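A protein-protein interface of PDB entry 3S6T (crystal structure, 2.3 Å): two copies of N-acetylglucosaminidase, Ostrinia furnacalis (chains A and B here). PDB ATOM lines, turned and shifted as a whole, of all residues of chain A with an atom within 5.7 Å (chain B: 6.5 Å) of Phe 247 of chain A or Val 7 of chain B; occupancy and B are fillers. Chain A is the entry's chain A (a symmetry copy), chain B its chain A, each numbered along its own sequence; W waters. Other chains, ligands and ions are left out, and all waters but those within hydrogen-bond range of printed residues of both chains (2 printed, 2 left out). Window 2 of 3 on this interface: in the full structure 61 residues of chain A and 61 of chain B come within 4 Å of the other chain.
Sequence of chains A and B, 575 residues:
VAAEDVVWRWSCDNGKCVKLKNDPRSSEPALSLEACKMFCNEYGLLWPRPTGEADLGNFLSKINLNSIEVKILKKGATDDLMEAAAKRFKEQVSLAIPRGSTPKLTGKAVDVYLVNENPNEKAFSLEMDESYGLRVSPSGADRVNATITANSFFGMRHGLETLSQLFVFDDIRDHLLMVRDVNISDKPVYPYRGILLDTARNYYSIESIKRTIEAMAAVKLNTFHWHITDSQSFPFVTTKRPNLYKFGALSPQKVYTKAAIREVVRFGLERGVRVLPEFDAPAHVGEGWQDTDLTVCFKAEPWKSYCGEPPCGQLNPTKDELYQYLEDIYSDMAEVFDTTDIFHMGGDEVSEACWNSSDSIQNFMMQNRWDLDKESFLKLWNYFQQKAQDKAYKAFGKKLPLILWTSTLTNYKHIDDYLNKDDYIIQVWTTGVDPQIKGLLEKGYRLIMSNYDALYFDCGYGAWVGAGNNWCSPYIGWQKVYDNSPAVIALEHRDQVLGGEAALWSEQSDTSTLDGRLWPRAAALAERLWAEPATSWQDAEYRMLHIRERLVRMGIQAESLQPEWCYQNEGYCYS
The side-chain amino group of Lys 246 of chain A is in salt-bridge range of the side-chain carboxylate of Glu 4 of chain B, at 3.9 Å. The indole nitrogen of Trp 8 of chain B lies within hydrogen-bond range of the backbone carbonyl oxygen of Phe 247 of chain A. NZ of Lys 19 of chain B lies within salt-bridge range of OE2 of Glu 287 of chain A (3.0 Å). NZ of Lys 21 of chain B is in salt-bridge range of OD2 of Asp 291 of chain A (2.8 Å).
The backbone carbonyl oxygen (O) of Val 7 of chain B lies within hydrogen-bond range of the backbone NH (N) of Asn 22 of chain B, at 3.3 Å. O of Lys 21 of chain B sits at hydrogen-bond distance from NE of Arg 9 of chain B (3.4 Å). The side-chain carboxylate (OE2) of Glu 287 of chain A sits close to the side-chain amide oxygen (OE1) of Gln 290 of chain A, 2.9 Å away. The backbone NH (N) of Gly 288 of chain A lies close to the side-chain amide nitrogen (NE2) of Gln 290 of chain A (3.0 Å).
Among the printed residues, merely in contact across the chains: Phe 247 of chain A with Lys 21 of chain B, Phe 247 of chain A with Val 7 of chain B, Lys 246 of chain A with Val 7 of chain B and Gln 290 of chain A with Trp 8 of chain B.
Printed residues of chain B within 4 Å of Lys 246 of chain A: Glu 4 and Val 7. Phe 247 of chain A touches just these residues of chain B: Val 7, Trp 8 and Lys 21. Printed residues of chain B within 4 Å of Gln 290 of chain A: Trp 8. Of the printed residues of chain B, Asp 291 of chain A touches Lys 21. Printed residues of chain A within 4 Å of Glu 4 of chain B: Lys 246. Val 7 of chain B touches just these residues of chain A: Lys 246 (3.6 Å) and Phe 247 (3.5 Å). Of the printed residues of chain A, Trp 8 of chain B touches Phe 247 and Gln 290. The nearest residue of chain B that does not touch Phe 247 of chain A is Lys 19 of chain B (4.5 Å).
Of the 12 printed residues of chain B, 5 touch a printed residue of chain A. Printed residues of chain A that touch a printed residue of chain B: Lys 246, Phe 247, Glu 287, Gln 290 and Asp 291. Hydrophobic or aromatic side chains of chain A that line the printed part of chain B: Phe 247. Among the printed residues, Asp or Glu carboxylates within 4 Å of a Lys or Arg side-chain nitrogen of the other chain: Lys 246 of chain A with Glu 4 of chain B (3.9 Å), Glu 287 of chain A with Lys 19 of chain B (3.0 Å) and Asp 291 of chain A with Lys 21 of chain B (2.8 Å).
No position is printed for both chains.
Water W2 lies within hydrogen-bond range of the backbone carbonyl oxygen (O) of Lys 246 of chain A (2.7 Å) and the backbone carbonyl oxygen (O) of Asp 5 of chain B (3.3 Å). Water W1 bridges OE1 of Glu 4 of chain B (2.8 Å) and NZ of Lys 246 of chain A (2.8 Å).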
ATOM      1  N   PRO A 242      -2.041   8.407 -16.991  1.00  0.00           N
ATOM      2  CA  PRO A 242      -1.477   9.074 -15.829  1.00  0.00           C
ATOM      3  C   PRO A 242      -2.204   8.925 -14.532  1.00  0.00           C
ATOM      4  O   PRO A 242      -1.576   9.049 -13.545  1.00  0.00           O
ATOM      5  CB  PRO A 242      -1.404  10.520 -16.270  1.00  0.00           C
ATOM      6  CG  PRO A 242      -2.324  10.631 -17.323  1.00  0.00           C
ATOM      7  CD  PRO A 242      -2.316   9.378 -18.045  1.00  0.00           C
ATOM      8  N   ASN A 243      -3.480   8.631 -14.538  1.00  0.00           N
ATOM      9  CA  ASN A 243      -4.205   8.429 -13.313  1.00  0.00           C
ATOM     10  C   ASN A 243      -3.784   7.233 -12.483  1.00  0.00           C
ATOM     11  O   ASN A 243      -4.008   7.218 -11.316  1.00  0.00           O
ATOM     12  CB  ASN A 243      -5.703   8.397 -13.539  1.00  0.00           C
ATOM     13  CG  ASN A 243      -6.268   9.727 -13.853  1.00  0.00           C
ATOM     14  OD1 ASN A 243      -5.625  10.745 -13.714  1.00  0.00           O
ATOM     15  ND2 ASN A 243      -7.505   9.733 -14.252  1.00  0.00           N
ATOM     16  N   LEU A 244      -3.218   6.219 -13.115  1.00  0.00           N
ATOM     17  CA  LEU A 244      -2.799   5.033 -12.417  1.00  0.00           C
ATOM     18  C   LEU A 244      -1.725   5.370 -11.427  1.00  0.00           C
ATOM     19  O   LEU A 244      -1.783   4.930 -10.340  1.00  0.00           O
ATOM     20  CB  LEU A 244      -2.338   3.945 -13.389  1.00  0.00           C
ATOM     21  CG  LEU A 244      -3.324   3.460 -14.436  1.00  0.00           C
ATOM     22  CD1 LEU A 244      -2.624   2.699 -15.493  1.00  0.00           C
ATOM     23  CD2 LEU A 244      -4.394   2.655 -13.816  1.00  0.00           C
ATOM     24  N   TYR A 245      -0.722   6.118 -11.829  1.00  0.00           N
ATOM     25  CA  TYR A 245       0.258   6.625 -10.911  1.00  0.00           C
ATOM     26  C   TYR A 245      -0.234   7.726  -9.989  1.00  0.00           C
ATOM     27  O   TYR A 245       0.166   7.799  -8.871  1.00  0.00           O
ATOM     28  CB  TYR A 245       1.583   6.944 -11.556  1.00  0.00           C
ATOM     29  CG  TYR A 245       1.672   8.229 -12.282  1.00  0.00           C
ATOM     30  CD1 TYR A 245       1.948   9.390 -11.630  1.00  0.00           C
ATOM     31  CD2 TYR A 245       1.532   8.277 -13.639  1.00  0.00           C
ATOM     32  CE1 TYR A 245       2.038  10.542 -12.300  1.00  0.00           C
ATOM     33  CE2 TYR A 245       1.631   9.423 -14.305  1.00  0.00           C
ATOM     34  CZ  TYR A 245       1.873  10.565 -13.636  1.00  0.00           C
ATOM     35  OH  TYR A 245       1.966  11.729 -14.311  1.00  0.00           O
ATOM     36  N   LYS A 246      -1.081   8.596 -10.495  1.00  0.00           N
ATOM     37  CA  LYS A 246      -1.573   9.648  -9.687  1.00  0.00           C
ATOM     38  C   LYS A 246      -2.364   9.101  -8.542  1.00  0.00           C
ATOM     39  O   LYS A 246      -2.152   9.491  -7.457  1.00  0.00           O
ATOM     40  CB  LYS A 246      -2.401  10.595 -10.523  1.00  0.00           C
ATOM     41  CG  LYS A 246      -2.982  11.753  -9.790  1.00  0.00           C
ATOM     42  CD  LYS A 246      -3.628  12.777 -10.726  1.00  0.00           C
ATOM     43  CE  LYS A 246      -4.611  13.650 -10.006  1.00  0.00           C
ATOM     44  NZ  LYS A 246      -5.573  14.292 -10.897  1.00  0.00           N
ATOM     45  N   PHE A 247      -3.316   8.236  -8.794  1.00  0.00           N
ATOM     46  CA  PHE A 247      -4.042   7.553  -7.748  1.00  0.00           C
ATOM     47  C   PHE A 247      -3.285   6.451  -7.024  1.00  0.00           C
ATOM     48  O   PHE A 247      -3.492   6.198  -5.888  1.00  0.00           O
ATOM     49  CB  PHE A 247      -5.419   7.095  -8.206  1.00  0.00           C
ATOM     50  CG  PHE A 247      -6.255   8.180  -8.767  1.00  0.00           C
ATOM     51  CD1 PHE A 247      -7.157   7.943  -9.757  1.00  0.00           C
ATOM     52  CD2 PHE A 247      -6.141   9.449  -8.315  1.00  0.00           C
ATOM     53  CE1 PHE A 247      -7.894   8.954 -10.255  1.00  0.00           C
ATOM     54  CE2 PHE A 247      -6.885  10.447  -8.826  1.00  0.00           C
ATOM     55  CZ  PHE A 247      -7.739  10.207  -9.781  1.00  0.00           C
ATOM     56  N   GLY A 248      -2.473   5.756  -7.791  1.00  0.00           N
ATOM     57  CA  GLY A 248      -1.681   4.612  -7.411  1.00  0.00           C
ATOM     58  C   GLY A 248      -0.517   4.694  -6.473  1.00  0.00           C
ATOM     59  O   GLY A 248      -0.281   3.806  -5.749  1.00  0.00           O
ATOM     60  N   ALA A 249       0.232   5.760  -6.555  1.00  0.00           N
ATOM     61  CA  ALA A 249       1.416   5.939  -5.780  1.00  0.00           C
ATOM     62  C   ALA A 249       1.184   6.166  -4.312  1.00  0.00           C
ATOM     63  O   ALA A 249       0.207   6.695  -3.930  1.00  0.00           O
ATOM     64  CB  ALA A 249       2.187   7.008  -6.331  1.00  0.00           C
ATOM     65  N   GLU A 287      -4.484  -0.512  -6.488  1.00  0.00           N
ATOM     66  CA  GLU A 287      -4.342   0.896  -6.428  1.00  0.00           C
ATOM     67  C   GLU A 287      -3.955   1.456  -7.775  1.00  0.00           C
ATOM     68  O   GLU A 287      -3.113   0.942  -8.446  1.00  0.00           O
ATOM     69  CB  GLU A 287      -3.306   1.253  -5.372  1.00  0.00           C
ATOM     70  CG  GLU A 287      -3.726   1.051  -3.962  1.00  0.00           C
ATOM     71  CD  GLU A 287      -4.595   2.164  -3.393  1.00  0.00           C
ATOM     72  OE1 GLU A 287      -5.138   1.989  -2.322  1.00  0.00           O
ATOM     73  OE2 GLU A 287      -4.751   3.192  -4.010  1.00  0.00           O
ATOM     74  N   GLY A 288      -4.589   2.558  -8.110  1.00  0.00           N
ATOM     75  CA  GLY A 288      -4.430   3.243  -9.359  1.00  0.00           C
ATOM     76  C   GLY A 288      -5.531   2.955 -10.332  1.00  0.00           C
ATOM     77  O   GLY A 288      -5.731   3.681 -11.235  1.00  0.00           O
ATOM     78  N   TRP A 289      -6.264   1.900 -10.107  1.00  0.00           N
ATOM     79  CA  TRP A 289      -7.347   1.521 -10.973  1.00  0.00           C
ATOM     80  C   TRP A 289      -8.726   1.993 -10.491  1.00  0.00           C
ATOM     81  O   TRP A 289      -9.692   1.667 -11.070  1.00  0.00           O
ATOM     82  CB  TRP A 289      -7.324   0.002 -11.238  1.00  0.00           C
ATOM     83  CG  TRP A 289      -6.105  -0.495 -11.937  1.00  0.00           C
ATOM     84  CD1 TRP A 289      -4.950  -0.871 -11.371  1.00  0.00           C
ATOM     85  CD2 TRP A 289      -5.938  -0.691 -13.330  1.00  0.00           C
ATOM     86  NE1 TRP A 289      -4.070  -1.263 -12.306  1.00  0.00           N
ATOM     87  CE2 TRP A 289      -4.653  -1.158 -13.528  1.00  0.00           C
ATOM     88  CE3 TRP A 289      -6.746  -0.499 -14.432  1.00  0.00           C
ATOM     89  CZ2 TRP A 289      -4.166  -1.432 -14.760  1.00  0.00           C
ATOM     90  CZ3 TRP A 289      -6.264  -0.775 -15.632  1.00  0.00           C
ATOM     91  CH2 TRP A 289      -4.991  -1.230 -15.802  1.00  0.00           C
ATOM     92  N   GLN A 290      -8.798   2.769  -9.437  1.00  0.00           N
ATOM     93  CA  GLN A 290     -10.074   3.231  -8.951  1.00  0.00           C
ATOM     94  C   GLN A 290     -10.785   4.083  -9.983  1.00  0.00           C
ATOM     95  O   GLN A 290     -10.198   4.903 -10.646  1.00  0.00           O
ATOM     96  CB  GLN A 290      -9.906   4.031  -7.670  1.00  0.00           C
ATOM     97  CG  GLN A 290      -9.366   3.254  -6.494  1.00  0.00           C
ATOM     98  CD  GLN A 290      -7.872   3.412  -6.250  1.00  0.00           C
ATOM     99  OE1 GLN A 290      -7.420   3.183  -5.181  1.00  0.00           O
ATOM    100  NE2 GLN A 290      -7.141   3.800  -7.234  1.00  0.00           N
ATOM    101  N   ASP A 291     -12.070   3.847 -10.119  1.00  0.00           N
ATOM    102  CA  ASP A 291     -12.891   4.600 -11.041  1.00  0.00           C
ATOM    103  C   ASP A 291     -12.778   4.184 -12.493  1.00  0.00           C
ATOM    104  O   ASP A 291     -13.324   4.833 -13.333  1.00  0.00           O
ATOM    105  CB  ASP A 291     -12.645   6.106 -10.942  1.00  0.00           C
ATOM    106  CG  ASP A 291     -12.968   6.672  -9.587  1.00  0.00           C
ATOM    107  OD1 ASP A 291     -14.064   6.413  -9.079  1.00  0.00           O
ATOM    108  OD2 ASP A 291     -12.126   7.394  -9.036  1.00  0.00           O
ATOM    109  N   GLU B   4       2.768  15.555  -9.256  1.00  0.00           N
ATOM    110  CA  GLU B   4       1.452  15.655  -8.786  1.00  0.00           C
ATOM    111  C   GLU B   4       1.425  16.151  -7.335  1.00  0.00           C
ATOM    112  O   GLU B   4       2.416  16.409  -6.724  1.00  0.00           O
ATOM    113  CB  GLU B   4       0.863  14.251  -8.931  1.00  0.00           C
ATOM    114  CG  GLU B   4      -0.576  14.177  -9.299  1.00  0.00           C
ATOM    115  CD  GLU B   4      -0.876  14.620 -10.723  1.00  0.00           C
ATOM    116  OE1 GLU B   4      -1.862  15.334 -10.930  1.00  0.00           O
ATOM    117  OE2 GLU B   4      -0.154  14.239 -11.638  1.00  0.00           O
ATOM    118  N   ASP B   5       0.231  16.292  -6.849  1.00  0.00           N
ATOM    119  CA  ASP B   5      -0.168  16.648  -5.490  1.00  0.00           C
ATOM    120  C   ASP B   5      -0.865  15.519  -4.828  1.00  0.00           C
ATOM    121  O   ASP B   5      -1.375  14.675  -5.501  1.00  0.00           O
ATOM    122  CB  ASP B   5      -1.187  17.762  -5.506  1.00  0.00           C
ATOM    123  CG  ASP B   5      -0.580  19.121  -5.679  1.00  0.00           C
ATOM    124  OD1 ASP B   5      -1.108  19.878  -6.501  1.00  0.00           O
ATOM    125  OD2 ASP B   5       0.376  19.441  -4.964  1.00  0.00           O
ATOM    126  N   VAL B   6      -0.903  15.486  -3.506  1.00  0.00           N
ATOM    127  CA  VAL B   6      -1.606  14.396  -2.897  1.00  0.00           C
ATOM    128  C   VAL B   6      -3.073  14.505  -3.175  1.00  0.00           C
ATOM    129  O   VAL B   6      -3.674  15.540  -3.115  1.00  0.00           O
ATOM    130  CB  VAL B   6      -1.183  14.043  -1.461  1.00  0.00           C
ATOM    131  CG1 VAL B   6      -0.176  14.966  -0.964  1.00  0.00           C
ATOM    132  CG2 VAL B   6      -2.343  13.973  -0.561  1.00  0.00           C
ATOM    133  N   VAL B   7      -3.587  13.375  -3.577  1.00  0.00           N
ATOM    134  CA  VAL B   7      -4.893  13.197  -4.093  1.00  0.00           C
ATOM    135  C   VAL B   7      -5.900  12.604  -3.149  1.00  0.00           C
ATOM    136  O   VAL B   7      -7.053  12.614  -3.426  1.00  0.00           O
ATOM    137  CB  VAL B   7      -4.718  12.269  -5.272  1.00  0.00           C
ATOM    138  CG1 VAL B   7      -5.753  11.279  -5.308  1.00  0.00           C
ATOM    139  CG2 VAL B   7      -4.675  13.040  -6.506  1.00  0.00           C
ATOM    140  N   TRP B   8      -5.440  12.099  -2.029  1.00  0.00           N
ATOM    141  CA  TRP B   8      -6.270  11.426  -1.057  1.00  0.00           C
ATOM    142  C   TRP B   8      -6.505  12.189   0.246  1.00  0.00           C
ATOM    143  O   TRP B   8      -5.851  13.118   0.530  1.00  0.00           O
ATOM    144  CB  TRP B   8      -5.699  10.047  -0.739  1.00  0.00           C
ATOM    145  CG  TRP B   8      -5.500   9.127  -1.896  1.00  0.00           C
ATOM    146  CD1 TRP B   8      -4.355   8.866  -2.507  1.00  0.00           C
ATOM    147  CD2 TRP B   8      -6.481   8.343  -2.553  1.00  0.00           C
ATOM    148  NE1 TRP B   8      -4.530   7.987  -3.497  1.00  0.00           N
ATOM    149  CE2 TRP B   8      -5.837   7.641  -3.552  1.00  0.00           C
ATOM    150  CE3 TRP B   8      -7.843   8.165  -2.392  1.00  0.00           C
ATOM    151  CZ2 TRP B   8      -6.495   6.789  -4.385  1.00  0.00           C
ATOM    152  CZ3 TRP B   8      -8.486   7.331  -3.220  1.00  0.00           C
ATOM    153  CH2 TRP B   8      -7.827   6.653  -4.204  1.00  0.00           C
ATOM    154  N   ARG B   9      -7.474  11.753   1.018  1.00  0.00           N
ATOM    155  CA  ARG B   9      -7.781  12.319   2.313  1.00  0.00           C
ATOM    156  C   ARG B   9      -8.157  11.198   3.224  1.00  0.00           C
ATOM    157  O   ARG B   9      -8.349  10.104   2.804  1.00  0.00           O
ATOM    158  CB  ARG B   9      -8.852  13.402   2.265  1.00  0.00           C
ATOM    159  CG  ARG B   9     -10.159  12.930   1.882  1.00  0.00           C
ATOM    160  CD  ARG B   9     -11.183  13.936   2.112  1.00  0.00           C
ATOM    161  NE  ARG B   9     -12.461  13.445   1.699  1.00  0.00           N
ATOM    162  CZ  ARG B   9     -13.344  12.903   2.490  1.00  0.00           C
ATOM    163  NH1 ARG B   9     -13.118  12.787   3.755  1.00  0.00           N
ATOM    164  NH2 ARG B   9     -14.456  12.480   1.992  1.00  0.00           N
ATOM    165  N   LYS B  19      -8.870   5.828   3.824  1.00  0.00           N
ATOM    166  CA  LYS B  19      -8.518   6.619   2.679  1.00  0.00           C
ATOM    167  C   LYS B  19      -9.672   6.793   1.728  1.00  0.00           C
ATOM    168  O   LYS B  19     -10.289   5.857   1.317  1.00  0.00           O
ATOM    169  CB  LYS B  19      -7.316   6.020   1.959  1.00  0.00           C
ATOM    170  CG  LYS B  19      -6.644   6.919   1.009  1.00  0.00           C
ATOM    171  CD  LYS B  19      -5.484   6.286   0.346  1.00  0.00           C
ATOM    172  CE  LYS B  19      -5.862   5.391  -0.798  1.00  0.00           C
ATOM    173  NZ  LYS B  19      -4.799   5.117  -1.710  1.00  0.00           N
ATOM    174  N   LEU B  20      -9.943   8.040   1.413  1.00  0.00           N
ATOM    175  CA  LEU B  20     -11.032   8.436   0.573  1.00  0.00           C
ATOM    176  C   LEU B  20     -10.509   9.437  -0.368  1.00  0.00           C
ATOM    177  O   LEU B  20      -9.567  10.083  -0.081  1.00  0.00           O
ATOM    178  CB  LEU B  20     -12.118   9.072   1.399  1.00  0.00           C
ATOM    179  CG  LEU B  20     -12.772   8.195   2.432  1.00  0.00           C
ATOM    180  CD1 LEU B  20     -13.529   9.045   3.339  1.00  0.00           C
ATOM    181  CD2 LEU B  20     -13.674   7.247   1.773  1.00  0.00           C
ATOM    182  N   LYS B  21     -11.130   9.561  -1.510  1.00  0.00           N
ATOM    183  CA  LYS B  21     -10.705  10.533  -2.468  1.00  0.00           C
ATOM    184  C   LYS B  21     -11.002  11.945  -1.995  1.00  0.00           C
ATOM    185  O   LYS B  21     -12.020  12.188  -1.430  1.00  0.00           O
ATOM    186  CB  LYS B  21     -11.355  10.265  -3.810  1.00  0.00           C
ATOM    187  CG  LYS B  21     -10.800  11.070  -4.929  1.00  0.00           C
ATOM    188  CD  LYS B  21      -9.867  10.264  -5.757  1.00  0.00           C
ATOM    189  CE  LYS B  21     -10.578   9.040  -6.321  1.00  0.00           C
ATOM    190  NZ  LYS B  21     -10.023   8.574  -7.591  1.00  0.00           N
ATOM    191  N   ASN B  22     -10.085  12.865  -2.215  1.00  0.00           N
ATOM    192  CA  ASN B  22     -10.318  14.236  -1.840  1.00  0.00           C
ATOM    193  C   ASN B  22     -11.053  14.959  -2.937  1.00  0.00           C
ATOM    194  O   ASN B  22     -10.462  15.642  -3.711  1.00  0.00           O
ATOM    195  CB  ASN B  22      -9.014  14.938  -1.557  1.00  0.00           C
ATOM    196  CG  ASN B  22      -9.207  16.261  -0.917  1.00  0.00           C
ATOM    197  OD1 ASN B  22      -8.313  17.051  -0.858  1.00  0.00           O
ATOM    198  ND2 ASN B  22     -10.381  16.497  -0.419  1.00  0.00           N
ATOM    199  N   ASP B  23     -12.352  14.754  -2.994  1.00  0.00           N
ATOM    200  CA  ASP B  23     -13.204  15.329  -4.006  1.00  0.00           C
ATOM    201  C   ASP B  23     -13.410  16.828  -3.843  1.00  0.00           C
ATOM    202  O   ASP B  23     -13.501  17.315  -2.768  1.00  0.00           O
ATOM    203  CB  ASP B  23     -14.536  14.587  -4.043  1.00  0.00           C
ATOM    204  CG  ASP B  23     -14.457  13.269  -4.781  1.00  0.00           C
ATOM    205  OD1 ASP B  23     -15.178  12.349  -4.398  1.00  0.00           O
ATOM    206  OD2 ASP B  23     -13.690  13.151  -5.746  1.00  0.00           O
ATOM    207  N   ILE B 172      -1.036  17.794   2.372  1.00  0.00           N
ATOM    208  CA  ILE B 172      -2.046  18.312   1.502  1.00  0.00           C
ATOM    209  C   ILE B 172      -1.907  19.815   1.309  1.00  0.00           C
ATOM    210  O   ILE B 172      -2.045  20.298   0.247  1.00  0.00           O
ATOM    211  CB  ILE B 172      -3.435  17.973   1.978  1.00  0.00           C
ATOM    212  CG1 ILE B 172      -3.696  16.497   1.829  1.00  0.00           C
ATOM    213  CG2 ILE B 172      -4.406  18.696   1.192  1.00  0.00           C
ATOM    214  CD1 ILE B 172      -4.824  16.049   2.534  1.00  0.00           C
HETATM  215  O   HOH W   1      -4.125  16.358 -12.215  1.00  0.00           O
HETATM  216  O   HOH W   2      -0.663  11.518  -6.345  1.00  0.00           O
